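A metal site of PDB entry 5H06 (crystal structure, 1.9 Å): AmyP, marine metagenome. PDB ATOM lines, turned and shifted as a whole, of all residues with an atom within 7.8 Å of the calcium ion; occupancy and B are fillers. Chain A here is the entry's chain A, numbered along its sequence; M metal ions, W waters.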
ATOM      1  N   ARG A 301      23.311   7.589  -7.182  1.00  0.00           N
ATOM      2  CA  ARG A 301      22.660   8.079  -5.973  1.00  0.00           C
ATOM      3  C   ARG A 301      21.647   7.075  -5.447  1.00  0.00           C
ATOM      4  O   ARG A 301      20.957   6.408  -6.224  1.00  0.00           O
ATOM      5  CB  ARG A 301      21.972   9.426  -6.226  1.00  0.00           C
ATOM      6  CG  ARG A 301      22.942  10.608  -6.257  1.00  0.00           C
ATOM      7  CD  ARG A 301      22.185  11.951  -6.280  1.00  0.00           C
ATOM      8  NE  ARG A 301      23.114  13.087  -6.260  1.00  0.00           N
ATOM      9  CZ  ARG A 301      23.784  13.490  -5.176  1.00  0.00           C
ATOM     10  NH1 ARG A 301      24.613  14.525  -5.257  1.00  0.00           N
ATOM     11  NH2 ARG A 301      23.618  12.860  -4.020  1.00  0.00           N
ATOM     12  N   GLY A 303      18.755   7.483  -4.149  1.00  0.00           N
ATOM     13  CA  GLY A 303      17.393   7.733  -4.632  1.00  0.00           C
ATOM     14  C   GLY A 303      17.175   7.337  -6.076  1.00  0.00           C
ATOM     15  O   GLY A 303      16.059   6.947  -6.458  1.00  0.00           O
ATOM     16  N   ASP A 304      18.204   7.449  -6.904  1.00  0.00           N
ATOM     17  CA  ASP A 304      18.084   6.931  -8.266  1.00  0.00           C
ATOM     18  C   ASP A 304      18.093   5.414  -8.283  1.00  0.00           C
ATOM     19  O   ASP A 304      17.414   4.800  -9.121  1.00  0.00           O
ATOM     20  CB  ASP A 304      19.186   7.511  -9.155  1.00  0.00           C
ATOM     21  CG  ASP A 304      18.966   8.977  -9.473  1.00  0.00           C
ATOM     22  OD1 ASP A 304      17.809   9.340  -9.770  1.00  0.00           O
ATOM     23  OD2 ASP A 304      19.931   9.777  -9.422  1.00  0.00           O
ATOM     24  N   LEU A 305      18.850   4.788  -7.370  1.00  0.00           N
ATOM     25  CA  LEU A 305      18.780   3.335  -7.236  1.00  0.00           C
ATOM     26  C   LEU A 305      17.386   2.878  -6.862  1.00  0.00           C
ATOM     27  O   LEU A 305      16.927   1.823  -7.314  1.00  0.00           O
ATOM     28  CB  LEU A 305      19.783   2.832  -6.187  1.00  0.00           C
ATOM     29  CG  LEU A 305      21.247   2.903  -6.630  1.00  0.00           C
ATOM     30  CD1 LEU A 305      22.178   2.556  -5.477  1.00  0.00           C
ATOM     31  CD2 LEU A 305      21.474   1.977  -7.848  1.00  0.00           C
ATOM     32  N   GLN A 307      14.572   4.344  -7.719  1.00  0.00           N
ATOM     33  CA  GLN A 307      13.756   4.442  -8.913  1.00  0.00           C
ATOM     34  C   GLN A 307      14.146   3.376  -9.938  1.00  0.00           C
ATOM     35  O   GLN A 307      13.285   2.807 -10.617  1.00  0.00           O
ATOM     36  CB  GLN A 307      13.885   5.846  -9.522  1.00  0.00           C
ATOM     37  CG  GLN A 307      13.297   6.961  -8.666  1.00  0.00           C
ATOM     38  CD  GLN A 307      13.564   8.340  -9.248  1.00  0.00           C
ATOM     39  OE1 GLN A 307      14.706   8.698  -9.554  1.00  0.00           O
ATOM     40  NE2 GLN A 307      12.500   9.127  -9.395  1.00  0.00           N
ATOM     41  N   ARG A 308      15.450   3.114 -10.066  1.00  0.00           N
ATOM     42  CA  ARG A 308      15.931   2.124 -11.015  1.00  0.00           C
ATOM     43  C   ARG A 308      15.346   0.751 -10.729  1.00  0.00           C
ATOM     44  O   ARG A 308      15.004  -0.005 -11.648  1.00  0.00           O
ATOM     45  CB  ARG A 308      17.461   2.056 -10.999  1.00  0.00           C
ATOM     46  CG  ARG A 308      18.030   0.892 -11.805  1.00  0.00           C
ATOM     47  CD  ARG A 308      19.576   0.882 -11.835  1.00  0.00           C
ATOM     48  NE  ARG A 308      20.112   2.103 -12.453  1.00  0.00           N
ATOM     49  CZ  ARG A 308      21.393   2.275 -12.749  1.00  0.00           C
ATOM     50  NH1 ARG A 308      21.798   3.420 -13.303  1.00  0.00           N
ATOM     51  NH2 ARG A 308      22.284   1.307 -12.511  1.00  0.00           N
ATOM     52  N   SER A 313       9.898   6.374  -5.550  1.00  0.00           N
ATOM     53  CA  SER A 313      10.294   7.648  -6.120  1.00  0.00           C
ATOM     54  C   SER A 313       9.894   8.745  -5.135  1.00  0.00           C
ATOM     55  O   SER A 313       9.076   8.491  -4.242  1.00  0.00           O
ATOM     56  CB  SER A 313       9.649   7.880  -7.493  1.00  0.00           C
ATOM     57  OG  SER A 313       8.240   7.969  -7.407  1.00  0.00           O
ATOM     58  N   PRO A 314      10.457   9.954  -5.265  1.00  0.00           N
ATOM     59  CA  PRO A 314      10.282  10.968  -4.202  1.00  0.00           C
ATOM     60  C   PRO A 314       8.833  11.331  -3.903  1.00  0.00           C
ATOM     61  O   PRO A 314       8.571  11.885  -2.822  1.00  0.00           O
ATOM     62  CB  PRO A 314      11.046  12.186  -4.751  1.00  0.00           C
ATOM     63  CG  PRO A 314      12.076  11.597  -5.636  1.00  0.00           C
ATOM     64  CD  PRO A 314      11.415  10.425  -6.288  1.00  0.00           C
ATOM     65  N   TYR A 319       9.915   6.120  -0.249  1.00  0.00           N
ATOM     66  CA  TYR A 319      11.199   6.649  -0.690  1.00  0.00           C
ATOM     67  C   TYR A 319      11.978   7.266   0.473  1.00  0.00           C
ATOM     68  O   TYR A 319      13.178   7.015   0.629  1.00  0.00           O
ATOM     69  CB  TYR A 319      10.961   7.695  -1.774  1.00  0.00           C
ATOM     70  CG  TYR A 319      12.183   8.382  -2.356  1.00  0.00           C
ATOM     71  CD1 TYR A 319      12.673   9.555  -1.794  1.00  0.00           C
ATOM     72  CD2 TYR A 319      12.821   7.880  -3.490  1.00  0.00           C
ATOM     73  CE1 TYR A 319      13.778  10.214  -2.341  1.00  0.00           C
ATOM     74  CE2 TYR A 319      13.929   8.526  -4.033  1.00  0.00           C
ATOM     75  CZ  TYR A 319      14.400   9.684  -3.458  1.00  0.00           C
ATOM     76  OH  TYR A 319      15.492  10.343  -3.993  1.00  0.00           O
ATOM     77  N   ASP A 347      18.576  13.380  -2.591  1.00  0.00           N
ATOM     78  CA  ASP A 347      18.804  13.821  -3.966  1.00  0.00           C
ATOM     79  C   ASP A 347      18.650  12.684  -4.969  1.00  0.00           C
ATOM     80  O   ASP A 347      18.874  11.512  -4.669  1.00  0.00           O
ATOM     81  CB  ASP A 347      20.211  14.422  -4.120  1.00  0.00           C
ATOM     82  CG  ASP A 347      20.218  15.938  -4.031  1.00  0.00           C
ATOM     83  OD1 ASP A 347      19.126  16.534  -3.957  1.00  0.00           O
ATOM     84  OD2 ASP A 347      21.310  16.544  -4.046  1.00  0.00           O
ATOM     85  N   GLU A 348      18.267  13.046  -6.189  1.00  0.00           N
ATOM     86  CA  GLU A 348      18.145  12.118  -7.297  1.00  0.00           C
ATOM     87  C   GLU A 348      18.071  12.955  -8.561  1.00  0.00           C
ATOM     88  O   GLU A 348      17.566  14.067  -8.549  1.00  0.00           O
ATOM     89  CB  GLU A 348      16.916  11.200  -7.153  1.00  0.00           C
ATOM     90  CG  GLU A 348      15.564  11.911  -6.986  1.00  0.00           C
ATOM     91  CD  GLU A 348      14.936  12.335  -8.322  1.00  0.00           C
ATOM     92  OE1 GLU A 348      15.254  11.729  -9.361  1.00  0.00           O
ATOM     93  OE2 GLU A 348      14.112  13.267  -8.332  1.00  0.00           O
ATOM     94  N   LEU A 349      18.621  12.422  -9.637  1.00  0.00           N
ATOM     95  CA  LEU A 349      18.671  13.142 -10.895  1.00  0.00           C
ATOM     96  C   LEU A 349      17.309  13.061 -11.582  1.00  0.00           C
ATOM     97  O   LEU A 349      16.852  11.969 -11.951  1.00  0.00           O
ATOM     98  CB  LEU A 349      19.770  12.573 -11.788  1.00  0.00           C
ATOM     99  CG  LEU A 349      19.907  13.212 -13.162  1.00  0.00           C
ATOM    100  CD1 LEU A 349      20.056  14.727 -13.043  1.00  0.00           C
ATOM    101  CD2 LEU A 349      21.082  12.594 -13.905  1.00  0.00           C
ATOM    102  N   GLU A 350      16.662  14.210 -11.743  1.00  0.00           N
ATOM    103  CA  GLU A 350      15.383  14.268 -12.446  1.00  0.00           C
ATOM    104  C   GLU A 350      15.522  13.738 -13.871  1.00  0.00           C
ATOM    105  O   GLU A 350      16.489  14.040 -14.585  1.00  0.00           O
ATOM    106  CB  GLU A 350      14.857  15.700 -12.472  1.00  0.00           C
ATOM    107  CG  GLU A 350      13.743  15.908 -13.485  1.00  0.00           C
ATOM    108  CD  GLU A 350      13.395  17.371 -13.695  1.00  0.00           C
ATOM    109  OE1 GLU A 350      13.660  18.185 -12.779  1.00  0.00           O
ATOM    110  OE2 GLU A 350      12.873  17.712 -14.783  1.00  0.00           O
ATOM    111  N   GLY A 351      14.550  12.934 -14.289  1.00  0.00           N
ATOM    112  CA  GLY A 351      14.546  12.403 -15.640  1.00  0.00           C
ATOM    113  C   GLY A 351      15.439  11.211 -15.845  1.00  0.00           C
ATOM    114  O   GLY A 351      15.556  10.733 -16.981  1.00  0.00           O
ATOM    115  N   TYR A 352      16.055  10.688 -14.783  1.00  0.00           N
ATOM    116  CA  TYR A 352      17.040   9.630 -14.889  1.00  0.00           C
ATOM    117  C   TYR A 352      16.763   8.542 -13.857  1.00  0.00           C
ATOM    118  O   TYR A 352      16.394   8.852 -12.722  1.00  0.00           O
ATOM    119  CB  TYR A 352      18.460  10.189 -14.657  1.00  0.00           C
ATOM    120  CG  TYR A 352      19.488   9.098 -14.475  1.00  0.00           C
ATOM    121  CD1 TYR A 352      20.077   8.470 -15.573  1.00  0.00           C
ATOM    122  CD2 TYR A 352      19.836   8.662 -13.197  1.00  0.00           C
ATOM    123  CE1 TYR A 352      20.994   7.452 -15.399  1.00  0.00           C
ATOM    124  CE2 TYR A 352      20.739   7.645 -13.012  1.00  0.00           C
ATOM    125  CZ  TYR A 352      21.320   7.052 -14.111  1.00  0.00           C
ATOM    126  OH  TYR A 352      22.208   6.048 -13.918  1.00  0.00           O
ATOM    127  N   ALA A 353      16.941   7.281 -14.237  1.00  0.00           N
ATOM    128  CA  ALA A 353      16.963   6.206 -13.241  1.00  0.00           C
ATOM    129  C   ALA A 353      17.620   4.958 -13.812  1.00  0.00           C
ATOM    130  O   ALA A 353      18.601   4.445 -13.253  1.00  0.00           O
ATOM    131  CB  ALA A 353      15.555   5.868 -12.748  1.00  0.00           C
ATOM    132  N   GLN A 354      17.073   4.455 -14.915  1.00  0.00           N
ATOM    133  CA  GLN A 354      17.621   3.284 -15.561  1.00  0.00           C
ATOM    134  C   GLN A 354      19.033   3.562 -16.055  1.00  0.00           C
ATOM    135  O   GLN A 354      19.392   4.701 -16.381  1.00  0.00           O
ATOM    136  CB  GLN A 354      16.724   2.844 -16.727  1.00  0.00           C
ATOM    137  CG  GLN A 354      15.406   2.268 -16.270  1.00  0.00           C
ATOM    138  CD  GLN A 354      15.574   0.904 -15.621  1.00  0.00           C
ATOM    139  OE1 GLN A 354      16.144  -0.013 -16.227  1.00  0.00           O
ATOM    140  NE2 GLN A 354      15.081   0.758 -14.396  1.00  0.00           N
HETATM  141 CA    CA M   1      15.934  10.161 -10.857  1.00  0.00          CA
HETATM  142  O   HOH W   1      14.063  10.320 -12.269  1.00  0.00           O
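The calcium ion is bound by the side-chain carboxylate (OE1) of Glu 348 (2.3 Å), the backbone carbonyl oxygen (O) of Leu 349 (2.3 Å), the side-chain amide oxygen (OE1) of Gln 307 (2.3 Å), the side-chain carboxylate (OD1) of Asp 304 (2.3 Å), the backbone carbonyl oxygen (O) of Tyr 352 (2.3 Å) and water W1 (2.3 Å).
Within 4 Å of the calcium ion: Asp 304, Gln 307, Glu 348, Leu 349 and Tyr 352.
OH of Tyr 352 sits at hydrogen-bond distance from NH1 of Arg 308, 2.7 Å away.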
